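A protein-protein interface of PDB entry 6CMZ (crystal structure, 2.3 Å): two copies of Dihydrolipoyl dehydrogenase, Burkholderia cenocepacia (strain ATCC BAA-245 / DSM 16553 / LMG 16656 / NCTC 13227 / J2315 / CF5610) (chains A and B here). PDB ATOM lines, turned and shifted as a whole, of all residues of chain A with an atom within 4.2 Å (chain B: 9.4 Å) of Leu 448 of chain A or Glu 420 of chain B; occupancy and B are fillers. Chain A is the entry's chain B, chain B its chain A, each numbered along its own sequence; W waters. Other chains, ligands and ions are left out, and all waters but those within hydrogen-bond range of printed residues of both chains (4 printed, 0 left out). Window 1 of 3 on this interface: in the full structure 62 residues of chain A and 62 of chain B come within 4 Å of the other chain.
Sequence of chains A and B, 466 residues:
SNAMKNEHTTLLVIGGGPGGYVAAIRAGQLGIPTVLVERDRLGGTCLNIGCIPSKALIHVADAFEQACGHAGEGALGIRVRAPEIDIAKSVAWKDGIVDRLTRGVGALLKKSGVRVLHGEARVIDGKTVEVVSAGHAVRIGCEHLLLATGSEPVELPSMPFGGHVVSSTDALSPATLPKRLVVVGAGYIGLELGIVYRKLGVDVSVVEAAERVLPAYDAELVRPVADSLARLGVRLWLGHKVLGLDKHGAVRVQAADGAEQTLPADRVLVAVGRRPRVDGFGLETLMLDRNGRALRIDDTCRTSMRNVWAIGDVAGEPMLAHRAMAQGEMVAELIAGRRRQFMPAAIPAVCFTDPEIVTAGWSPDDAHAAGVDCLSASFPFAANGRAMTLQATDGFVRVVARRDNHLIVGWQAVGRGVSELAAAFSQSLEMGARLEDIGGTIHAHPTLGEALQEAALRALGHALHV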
ATOM      1  N   PHE A 381      20.554  20.362   5.004  1.00  0.00           N
ATOM      2  CA  PHE A 381      19.817  21.584   5.266  1.00  0.00           C
ATOM      3  C   PHE A 381      20.757  22.765   5.554  1.00  0.00           C
ATOM      4  O   PHE A 381      20.327  23.910   5.518  1.00  0.00           O
ATOM      5  CB  PHE A 381      18.769  21.396   6.358  1.00  0.00           C
ATOM      6  CG  PHE A 381      17.596  20.547   5.937  1.00  0.00           C
ATOM      7  CD1 PHE A 381      16.759  20.969   4.916  1.00  0.00           C
ATOM      8  CD2 PHE A 381      17.277  19.390   6.609  1.00  0.00           C
ATOM      9  CE1 PHE A 381      15.659  20.222   4.520  1.00  0.00           C
ATOM     10  CE2 PHE A 381      16.172  18.633   6.234  1.00  0.00           C
ATOM     11  CZ  PHE A 381      15.363  19.049   5.183  1.00  0.00           C
ATOM     12  N   ASN A 384      20.562  25.073   2.640  1.00  0.00           N
ATOM     13  CA  ASN A 384      19.203  25.402   2.220  1.00  0.00           C
ATOM     14  C   ASN A 384      18.881  26.755   2.863  1.00  0.00           C
ATOM     15  O   ASN A 384      19.053  26.927   4.076  1.00  0.00           O
ATOM     16  CB  ASN A 384      18.270  24.299   2.721  1.00  0.00           C
ATOM     17  CG  ASN A 384      16.806  24.577   2.444  1.00  0.00           C
ATOM     18  OD1 ASN A 384      16.124  25.106   3.306  1.00  0.00           O
ATOM     19  ND2 ASN A 384      16.327  24.249   1.238  1.00  0.00           N
ATOM     20  N   ARG A 386      15.967  28.375   3.390  1.00  0.00           N
ATOM     21  CA  ARG A 386      14.846  28.357   4.310  1.00  0.00           C
ATOM     22  C   ARG A 386      15.261  27.851   5.685  1.00  0.00           C
ATOM     23  O   ARG A 386      14.914  28.460   6.714  1.00  0.00           O
ATOM     24  CB  ARG A 386      13.696  27.529   3.729  1.00  0.00           C
ATOM     25  CG  ARG A 386      12.442  27.474   4.578  1.00  0.00           C
ATOM     26  CD  ARG A 386      11.919  28.855   4.915  1.00  0.00           C
ATOM     27  NE  ARG A 386      10.679  28.783   5.683  1.00  0.00           N
ATOM     28  CZ  ARG A 386      10.190  29.765   6.433  1.00  0.00           C
ATOM     29  NH1 ARG A 386       9.053  29.568   7.085  1.00  0.00           N
ATOM     30  NH2 ARG A 386      10.836  30.931   6.560  1.00  0.00           N
ATOM     31  N   ALA A 387      15.998  26.739   5.690  1.00  0.00           N
ATOM     32  CA  ALA A 387      16.506  26.155   6.922  1.00  0.00           C
ATOM     33  C   ALA A 387      17.286  27.190   7.722  1.00  0.00           C
ATOM     34  O   ALA A 387      17.124  27.279   8.930  1.00  0.00           O
ATOM     35  CB  ALA A 387      17.388  24.954   6.619  1.00  0.00           C
ATOM     36  N   ARG A 416      14.480  19.862  11.556  1.00  0.00           N
ATOM     37  CA  ARG A 416      13.360  20.456  12.284  1.00  0.00           C
ATOM     38  C   ARG A 416      12.311  20.858  11.259  1.00  0.00           C
ATOM     39  O   ARG A 416      12.643  21.335  10.176  1.00  0.00           O
ATOM     40  CB  ARG A 416      13.743  21.688  13.087  1.00  0.00           C
ATOM     41  CG  ARG A 416      14.883  21.515  14.072  1.00  0.00           C
ATOM     42  CD  ARG A 416      14.845  22.624  15.129  1.00  0.00           C
ATOM     43  NE  ARG A 416      13.685  22.450  16.015  1.00  0.00           N
ATOM     44  CZ  ARG A 416      13.317  23.289  16.985  1.00  0.00           C
ATOM     45  NH1 ARG A 416      12.245  23.008  17.723  1.00  0.00           N
ATOM     46  NH2 ARG A 416      14.004  24.404  17.224  1.00  0.00           N
ATOM     47  N   GLY A 417      11.050  20.640  11.601  1.00  0.00           N
ATOM     48  CA  GLY A 417       9.928  21.010  10.735  1.00  0.00           C
ATOM     49  C   GLY A 417       9.870  20.373   9.363  1.00  0.00           C
ATOM     50  O   GLY A 417       9.454  21.023   8.411  1.00  0.00           O
ATOM     51  N   LEU A 421       6.695  17.103   4.814  1.00  0.00           N
ATOM     52  CA  LEU A 421       7.258  16.559   3.568  1.00  0.00           C
ATOM     53  C   LEU A 421       6.717  15.140   3.356  1.00  0.00           C
ATOM     54  O   LEU A 421       6.801  14.597   2.249  1.00  0.00           O
ATOM     55  CB  LEU A 421       8.797  16.524   3.583  1.00  0.00           C
ATOM     56  CG  LEU A 421       9.503  17.886   3.652  1.00  0.00           C
ATOM     57  CD1 LEU A 421      11.018  17.744   3.703  1.00  0.00           C
ATOM     58  CD2 LEU A 421       9.073  18.752   2.474  1.00  0.00           C
ATOM     59  N   THR A 447      11.944  27.130   0.458  1.00  0.00           N
ATOM     60  CA  THR A 447      11.294  26.060   1.219  1.00  0.00           C
ATOM     61  C   THR A 447      12.279  24.946   1.531  1.00  0.00           C
ATOM     62  O   THR A 447      13.306  24.794   0.869  1.00  0.00           O
ATOM     63  CB  THR A 447      10.070  25.449   0.477  1.00  0.00           C
ATOM     64  OG1 THR A 447      10.466  24.995  -0.815  1.00  0.00           O
ATOM     65  CG2 THR A 447       8.949  26.463   0.310  1.00  0.00           C
ATOM     66  N   LEU A 448      11.967  24.194   2.578  1.00  0.00           N
ATOM     67  CA  LEU A 448      12.766  23.021   2.961  1.00  0.00           C
ATOM     68  C   LEU A 448      12.622  21.994   1.837  1.00  0.00           C
ATOM     69  O   LEU A 448      13.559  21.270   1.527  1.00  0.00           O
ATOM     70  CB  LEU A 448      12.295  22.430   4.307  1.00  0.00           C
ATOM     71  CG  LEU A 448      12.446  23.350   5.535  1.00  0.00           C
ATOM     72  CD1 LEU A 448      11.797  22.760   6.777  1.00  0.00           C
ATOM     73  CD2 LEU A 448      13.913  23.644   5.794  1.00  0.00           C
ATOM     74  N   GLY A 449      11.438  21.975   1.222  1.00  0.00           N
ATOM     75  CA  GLY A 449      11.122  21.066   0.126  1.00  0.00           C
ATOM     76  C   GLY A 449      12.041  21.192  -1.063  1.00  0.00           C
ATOM     77  O   GLY A 449      12.140  20.271  -1.856  1.00  0.00           O
ATOM     78  N   GLU A 450      12.686  22.342  -1.224  1.00  0.00           N
ATOM     79  CA  GLU A 450      13.662  22.502  -2.316  1.00  0.00           C
ATOM     80  C   GLU A 450      14.773  21.469  -2.217  1.00  0.00           C
ATOM     81  O   GLU A 450      15.352  21.086  -3.236  1.00  0.00           O
ATOM     82  CB  GLU A 450      14.270  23.897  -2.328  1.00  0.00           C
ATOM     83  CG  GLU A 450      13.370  24.930  -2.981  1.00  0.00           C
ATOM     84  CD  GLU A 450      13.979  26.321  -2.958  1.00  0.00           C
ATOM     85  OE1 GLU A 450      14.081  26.903  -1.840  1.00  0.00           O
ATOM     86  OE2 GLU A 450      14.306  26.838  -4.070  1.00  0.00           O
ATOM     87  N   ALA A 451      15.060  21.017  -0.995  1.00  0.00           N
ATOM     88  CA  ALA A 451      16.095  20.004  -0.784  1.00  0.00           C
ATOM     89  C   ALA A 451      15.763  18.675  -1.489  1.00  0.00           C
ATOM     90  O   ALA A 451      16.671  17.923  -1.811  1.00  0.00           O
ATOM     91  CB  ALA A 451      16.343  19.779   0.702  1.00  0.00           C
ATOM     92  N   LYS B  55      11.986  36.460   4.833  1.00  0.00           N
ATOM     93  CA  LYS B  55      11.701  35.254   5.624  1.00  0.00           C
ATOM     94  C   LYS B  55      12.459  35.251   6.955  1.00  0.00           C
ATOM     95  O   LYS B  55      11.915  34.794   7.967  1.00  0.00           O
ATOM     96  CB  LYS B  55      11.926  33.967   4.815  1.00  0.00           C
ATOM     97  CG  LYS B  55      10.663  33.381   4.141  1.00  0.00           C
ATOM     98  CD  LYS B  55       9.695  34.365   3.464  1.00  0.00           C
ATOM     99  CE  LYS B  55      10.229  35.071   2.253  1.00  0.00           C
ATOM    100  NZ  LYS B  55       9.207  35.966   1.600  1.00  0.00           N
ATOM    101  N   ALA B 349       3.710  29.068  -5.447  1.00  0.00           N
ATOM    102  CA  ALA B 349       4.007  30.303  -4.767  1.00  0.00           C
ATOM    103  C   ALA B 349       3.606  30.203  -3.319  1.00  0.00           C
ATOM    104  O   ALA B 349       2.651  29.502  -2.976  1.00  0.00           O
ATOM    105  CB  ALA B 349       3.282  31.461  -5.438  1.00  0.00           C
ATOM    106  N   VAL B 350       4.365  30.884  -2.470  1.00  0.00           N
ATOM    107  CA  VAL B 350       4.083  30.924  -1.043  1.00  0.00           C
ATOM    108  C   VAL B 350       4.108  32.365  -0.583  1.00  0.00           C
ATOM    109  O   VAL B 350       5.101  33.097  -0.793  1.00  0.00           O
ATOM    110  CB  VAL B 350       5.092  30.123  -0.205  1.00  0.00           C
ATOM    111  CG1 VAL B 350       4.729  30.208   1.269  1.00  0.00           C
ATOM    112  CG2 VAL B 350       5.091  28.671  -0.637  1.00  0.00           C
ATOM    113  N   PHE B 352       4.159  34.385   2.574  1.00  0.00           N
ATOM    114  CA  PHE B 352       4.494  34.223   4.000  1.00  0.00           C
ATOM    115  C   PHE B 352       3.844  35.175   5.014  1.00  0.00           C
ATOM    116  O   PHE B 352       4.479  35.582   5.995  1.00  0.00           O
ATOM    117  CB  PHE B 352       6.006  34.176   4.180  1.00  0.00           C
ATOM    118  CG  PHE B 352       6.619  32.903   3.695  1.00  0.00           C
ATOM    119  CD1 PHE B 352       6.989  32.752   2.358  1.00  0.00           C
ATOM    120  CD2 PHE B 352       6.836  31.842   4.575  1.00  0.00           C
ATOM    121  CE1 PHE B 352       7.580  31.577   1.912  1.00  0.00           C
ATOM    122  CE2 PHE B 352       7.427  30.668   4.125  1.00  0.00           C
ATOM    123  CZ  PHE B 352       7.790  30.534   2.790  1.00  0.00           C
ATOM    124  N   GLU B 356      -0.299  31.868   6.268  1.00  0.00           N
ATOM    125  CA  GLU B 356       0.382  31.790   4.978  1.00  0.00           C
ATOM    126  C   GLU B 356      -0.591  31.321   3.911  1.00  0.00           C
ATOM    127  O   GLU B 356      -1.612  30.721   4.211  1.00  0.00           O
ATOM    128  CB  GLU B 356       1.533  30.775   5.047  1.00  0.00           C
ATOM    129  CG  GLU B 356       2.652  31.097   6.044  1.00  0.00           C
ATOM    130  CD  GLU B 356       3.590  29.912   6.288  1.00  0.00           C
ATOM    131  OE1 GLU B 356       3.169  28.765   6.014  1.00  0.00           O
ATOM    132  OE2 GLU B 356       4.730  30.103   6.784  1.00  0.00           O
ATOM    133  N   ILE B 357      -0.250  31.598   2.663  1.00  0.00           N
ATOM    134  CA  ILE B 357      -1.047  31.157   1.521  1.00  0.00           C
ATOM    135  C   ILE B 357      -0.099  30.413   0.601  1.00  0.00           C
ATOM    136  O   ILE B 357       0.978  30.928   0.276  1.00  0.00           O
ATOM    137  CB  ILE B 357      -1.718  32.323   0.769  1.00  0.00           C
ATOM    138  CG1 ILE B 357      -2.837  32.916   1.627  1.00  0.00           C
ATOM    139  CG2 ILE B 357      -2.282  31.847  -0.572  1.00  0.00           C
ATOM    140  CD1 ILE B 357      -3.482  34.154   1.026  1.00  0.00           C
ATOM    141  N   VAL B 358      -0.493  29.202   0.206  1.00  0.00           N
ATOM    142  CA  VAL B 358       0.304  28.385  -0.685  1.00  0.00           C
ATOM    143  C   VAL B 358      -0.550  28.059  -1.866  1.00  0.00           C
ATOM    144  O   VAL B 358      -1.715  27.682  -1.705  1.00  0.00           O
ATOM    145  CB  VAL B 358       0.726  27.047  -0.054  1.00  0.00           C
ATOM    146  CG1 VAL B 358       1.759  26.352  -0.940  1.00  0.00           C
ATOM    147  CG2 VAL B 358       1.316  27.261   1.318  1.00  0.00           C
ATOM    148  N   ALA B 413      -3.850  26.434  -0.357  1.00  0.00           N
ATOM    149  CA  ALA B 413      -3.949  26.211   1.069  1.00  0.00           C
ATOM    150  C   ALA B 413      -3.689  27.489   1.784  1.00  0.00           C
ATOM    151  O   ALA B 413      -2.851  28.293   1.343  1.00  0.00           O
ATOM    152  CB  ALA B 413      -2.961  25.151   1.527  1.00  0.00           C
ATOM    153  N   GLY B 415      -3.243  28.734   5.920  1.00  0.00           N
ATOM    154  CA  GLY B 415      -3.136  28.360   7.306  1.00  0.00           C
ATOM    155  C   GLY B 415      -1.751  28.665   7.839  1.00  0.00           C
ATOM    156  O   GLY B 415      -0.825  29.020   7.081  1.00  0.00           O
ATOM    157  N   ARG B 416      -1.610  28.515   9.152  1.00  0.00           N
ATOM    158  CA  ARG B 416      -0.352  28.753   9.815  1.00  0.00           C
ATOM    159  C   ARG B 416       0.530  27.518   9.612  1.00  0.00           C
ATOM    160  O   ARG B 416       0.100  26.389   9.828  1.00  0.00           O
ATOM    161  CB  ARG B 416      -0.612  29.067  11.285  1.00  0.00           C
ATOM    162  CG  ARG B 416       0.528  29.797  11.965  1.00  0.00           C
ATOM    163  CD  ARG B 416       0.043  30.567  13.185  1.00  0.00           C
ATOM    164  NE  ARG B 416      -0.250  29.716  14.332  1.00  0.00           N
ATOM    165  CZ  ARG B 416       0.567  29.520  15.374  1.00  0.00           C
ATOM    166  NH1 ARG B 416       0.184  28.720  16.371  1.00  0.00           N
ATOM    167  NH2 ARG B 416       1.756  30.124  15.447  1.00  0.00           N
ATOM    168  N   GLY B 417       1.744  27.748   9.124  1.00  0.00           N
ATOM    169  CA  GLY B 417       2.726  26.692   8.880  1.00  0.00           C
ATOM    170  C   GLY B 417       2.386  25.707   7.773  1.00  0.00           C
ATOM    171  O   GLY B 417       2.676  24.510   7.912  1.00  0.00           O
ATOM    172  N   VAL B 418       1.777  26.184   6.686  1.00  0.00           N
ATOM    173  CA  VAL B 418       1.412  25.289   5.571  1.00  0.00           C
ATOM    174  C   VAL B 418       2.363  25.378   4.377  1.00  0.00           C
ATOM    175  O   VAL B 418       2.155  24.701   3.379  1.00  0.00           O
ATOM    176  CB  VAL B 418      -0.032  25.542   5.055  1.00  0.00           C
ATOM    177  CG1 VAL B 418      -1.060  25.311   6.163  1.00  0.00           C
ATOM    178  CG2 VAL B 418      -0.182  26.946   4.469  1.00  0.00           C
ATOM    179  N   SER B 419       3.411  26.196   4.488  1.00  0.00           N
ATOM    180  CA  SER B 419       4.338  26.412   3.376  1.00  0.00           C
ATOM    181  C   SER B 419       4.949  25.143   2.802  1.00  0.00           C
ATOM    182  O   SER B 419       5.018  24.992   1.578  1.00  0.00           O
ATOM    183  CB  SER B 419       5.464  27.390   3.783  1.00  0.00           C
ATOM    184  OG  SER B 419       6.222  26.883   4.857  1.00  0.00           O
ATOM    185  N   GLU B 420       5.366  24.228   3.676  1.00  0.00           N
ATOM    186  CA  GLU B 420       6.014  22.981   3.246  1.00  0.00           C
ATOM    187  C   GLU B 420       5.134  22.016   2.462  1.00  0.00           C
ATOM    188  O   GLU B 420       5.651  21.071   1.856  1.00  0.00           O
ATOM    189  CB  GLU B 420       6.753  22.307   4.406  1.00  0.00           C
ATOM    190  CG  GLU B 420       7.904  23.153   4.968  1.00  0.00           C
ATOM    191  CD  GLU B 420       8.976  23.497   3.923  1.00  0.00           C
ATOM    192  OE1 GLU B 420       9.173  22.743   2.938  1.00  0.00           O
ATOM    193  OE2 GLU B 420       9.658  24.533   4.086  1.00  0.00           O
ATOM    194  N   LEU B 421       3.821  22.264   2.435  1.00  0.00           N
ATOM    195  CA  LEU B 421       2.902  21.468   1.586  1.00  0.00           C
ATOM    196  C   LEU B 421       3.156  21.775   0.102  1.00  0.00           C
ATOM    197  O   LEU B 421       2.649  21.083  -0.768  1.00  0.00           O
ATOM    198  CB  LEU B 421       1.437  21.760   1.899  1.00  0.00           C
ATOM    199  CG  LEU B 421       0.897  21.320   3.263  1.00  0.00           C
ATOM    200  CD1 LEU B 421      -0.536  21.789   3.415  1.00  0.00           C
ATOM    201  CD2 LEU B 421       0.969  19.812   3.439  1.00  0.00           C
ATOM    202  N   ALA B 422       3.918  22.840  -0.168  1.00  0.00           N
ATOM    203  CA  ALA B 422       4.235  23.257  -1.536  1.00  0.00           C
ATOM    204  C   ALA B 422       4.873  22.156  -2.348  1.00  0.00           C
ATOM    205  O   ALA B 422       4.588  22.028  -3.526  1.00  0.00           O
ATOM    206  CB  ALA B 422       5.134  24.476  -1.517  1.00  0.00           C
ATOM    207  N   ALA B 423       5.761  21.382  -1.719  1.00  0.00           N
ATOM    208  CA  ALA B 423       6.427  20.267  -2.386  1.00  0.00           C
ATOM    209  C   ALA B 423       5.386  19.239  -2.857  1.00  0.00           C
ATOM    210  O   ALA B 423       5.414  18.779  -4.011  1.00  0.00           O
ATOM    211  CB  ALA B 423       7.441  19.609  -1.455  1.00  0.00           C
ATOM    212  N   ALA B 424       4.490  18.872  -1.956  1.00  0.00           N
ATOM    213  CA  ALA B 424       3.429  17.922  -2.280  1.00  0.00           C
ATOM    214  C   ALA B 424       2.583  18.443  -3.450  1.00  0.00           C
ATOM    215  O   ALA B 424       2.363  17.715  -4.438  1.00  0.00           O
ATOM    216  CB  ALA B 424       2.551  17.668  -1.066  1.00  0.00           C
ATOM    217  N   PHE B 425       2.154  19.704  -3.372  1.00  0.00           N
ATOM    218  CA  PHE B 425       1.339  20.266  -4.456  1.00  0.00           C
ATOM    219  C   PHE B 425       2.061  20.294  -5.795  1.00  0.00           C
ATOM    220  O   PHE B 425       1.513  19.893  -6.827  1.00  0.00           O
ATOM    221  CB  PHE B 425       0.877  21.685  -4.172  1.00  0.00           C
ATOM    222  CG  PHE B 425       0.081  21.860  -2.916  1.00  0.00           C
ATOM    223  CD1 PHE B 425      -0.710  20.850  -2.395  1.00  0.00           C
ATOM    224  CD2 PHE B 425      -0.016  23.127  -2.353  1.00  0.00           C
ATOM    225  CE1 PHE B 425      -1.462  21.063  -1.262  1.00  0.00           C
ATOM    226  CE2 PHE B 425      -0.796  23.347  -1.221  1.00  0.00           C
ATOM    227  CZ  PHE B 425      -1.514  22.310  -0.675  1.00  0.00           C
ATOM    228  N   SER B 426       3.295  20.756  -5.773  1.00  0.00           N
ATOM    229  CA  SER B 426       4.065  20.901  -6.991  1.00  0.00           C
ATOM    230  C   SER B 426       4.385  19.548  -7.626  1.00  0.00           C
ATOM    231  O   SER B 426       4.205  19.358  -8.837  1.00  0.00           O
ATOM    232  CB  SER B 426       5.325  21.697  -6.696  1.00  0.00           C
ATOM    233  OG  SER B 426       5.967  22.058  -7.904  1.00  0.00           O
ATOM    234  N   GLN B 427       4.800  18.591  -6.804  1.00  0.00           N
ATOM    235  CA  GLN B 427       5.135  17.254  -7.296  1.00  0.00           C
ATOM    236  C   GLN B 427       3.924  16.469  -7.824  1.00  0.00           C
ATOM    237  O   GLN B 427       4.060  15.751  -8.824  1.00  0.00           O
ATOM    238  CB  GLN B 427       5.888  16.448  -6.232  1.00  0.00           C
ATOM    239  CG  GLN B 427       7.273  16.994  -5.925  1.00  0.00           C
ATOM    240  CD  GLN B 427       7.957  16.252  -4.797  1.00  0.00           C
ATOM    241  OE1 GLN B 427       7.545  15.152  -4.438  1.00  0.00           O
ATOM    242  NE2 GLN B 427       9.019  16.848  -4.232  1.00  0.00           N
ATOM    243  N   LEU B 448      -0.730  17.857   8.748  1.00  0.00           N
ATOM    244  CA  LEU B 448      -1.617  18.796   8.063  1.00  0.00           C
ATOM    245  C   LEU B 448      -1.951  18.197   6.697  1.00  0.00           C
ATOM    246  O   LEU B 448      -3.081  18.337   6.193  1.00  0.00           O
ATOM    247  CB  LEU B 448      -0.970  20.169   7.880  1.00  0.00           C
ATOM    248  CG  LEU B 448      -0.565  20.969   9.119  1.00  0.00           C
ATOM    249  CD1 LEU B 448       0.099  22.265   8.684  1.00  0.00           C
ATOM    250  CD2 LEU B 448      -1.765  21.247  10.009  1.00  0.00           C
ATOM    251  N   GLY B 449      -0.963  17.502   6.133  1.00  0.00           N
ATOM    252  CA  GLY B 449      -1.091  16.834   4.853  1.00  0.00           C
ATOM    253  C   GLY B 449      -2.318  15.957   4.694  1.00  0.00           C
ATOM    254  O   GLY B 449      -2.838  15.832   3.585  1.00  0.00           O
ATOM    255  N   LEU B 452      -5.154  17.183   2.598  1.00  0.00           N
ATOM    256  CA  LEU B 452      -5.108  17.047   1.127  1.00  0.00           C
ATOM    257  C   LEU B 452      -5.909  15.815   0.691  1.00  0.00           C
ATOM    258  O   LEU B 452      -6.694  15.879  -0.263  1.00  0.00           O
ATOM    259  CB  LEU B 452      -3.657  16.936   0.578  1.00  0.00           C
ATOM    260  CG  LEU B 452      -2.724  18.163   0.540  1.00  0.00           C
ATOM    261  CD1 LEU B 452      -2.499  18.772   1.896  1.00  0.00           C
ATOM    262  CD2 LEU B 452      -1.365  17.825  -0.066  1.00  0.00           C
HETATM  263  O   HOH W   1      10.208  32.711   8.645  1.00  0.00           O
HETATM  264  O   HOH W   2       8.932  27.012   4.800  1.00  0.00           O
HETATM  265  O   HOH W   3       8.660  22.926  -1.634  1.00  0.00           O
HETATM  266  O   HOH W   4       6.353  28.123   7.314  1.00  0.00           O
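N of Leu 448 of chain A sits at hydrogen-bond distance from OE2 of Glu 420 of chain B, at 2.8 Å.
OE1 of Glu 420 of chain B lies within hydrogen-bond range of N of Gly 449 of chain A.
The side-chain amide nitrogen of Asn 384 of chain A lies within hydrogen-bond range of the backbone carbonyl oxygen of Thr 447 of chain A (3.1 Å).
The backbone NH (N) of Arg 386 of chain A is in hydrogen-bond range of the side-chain amide oxygen (OD1) of Asn 384 of chain A, 3.3 Å away.
The side-chain carboxylate (OE1) of Glu 450 of chain A is in hydrogen-bond range of the backbone NH (N) of Thr 447 of chain A (3.1 Å).
Of the printed residues of chain A, Glu 420 of chain B touches Thr 447 (3.6 Å), Leu 448 (2.8 Å) and Gly 449 (2.9 Å).
No residue of chain B comes within 4 Å of Gly 417 of chain A.
Printed residues of chain B within 4 Å of Thr 447 of chain A: Glu 420.
Gly 449 of chain A touches just one residue of chain B: Glu 420.
Of the printed residues of chain A, Phe 352 of chain B touches Arg 386 (3.6 Å).
Printed residues of chain A within 4 Å of Lys 55 of chain B: Arg 386.
Of the printed residues of chain B, Arg 386 of chain A touches Lys 55 (3.4 Å) and Phe 352 (3.6 Å).
Leu 421 of chain B touches none of the printed residues of chain A.
The nearest residue of chain B that does not touch Leu 448 of chain A is Ala 423 of chain B (6.6 Å).
The nearest printed residue of chain A that does not touch Lys 55 of chain B is Thr 447 of chain A (7.4 Å).
Water W4 lies within hydrogen-bond range of OE2 of Glu 356 of chain B (2.6 Å), OG of Ser 419 of chain B (2.8 Å) and NH1 of Arg 386 of chain A (3.1 Å).
Water W2 lies within hydrogen-bond range of NE of Arg 386 of chain A (2.6 Å), OE2 of Glu 420 of chain B (2.7 Å) and OG of Ser 419 of chain B (2.7 Å).
Water W1 bridges O of Lys 55 of chain B (2.8 Å) and NH2 of Arg 386 of chain A (2.8 Å).
Water W3 lies within hydrogen-bond range of the side-chain hydroxyl (OG1) of Thr 447 of chain A (2.9 Å) and the backbone NH (N) of Ala 423 of chain B (3.3 Å).
Of the 12 printed residues of chain A, 4 touch a printed residue of chain B.
Printed residues of chain B that touch a printed residue of chain A: Lys 55, Phe 352 and Glu 420.
Hydrophobic or aromatic side chains of chain B that line the printed part of chain A: Phe 352.
Among the printed residues, no Asp or Glu carboxylate lies within 4 Å of a Lys or Arg side-chain nitrogen of the other chain.
Positions printed for both chains: 416, 417, 421, 448 and 449.
Among the printed residues, merely in contact across the chains: Arg 386 of chain A with Lys 55 of chain B, Arg 386 of chain A with Phe 352 of chain B and Thr 447 of chain A with Glu 420 of chain B.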
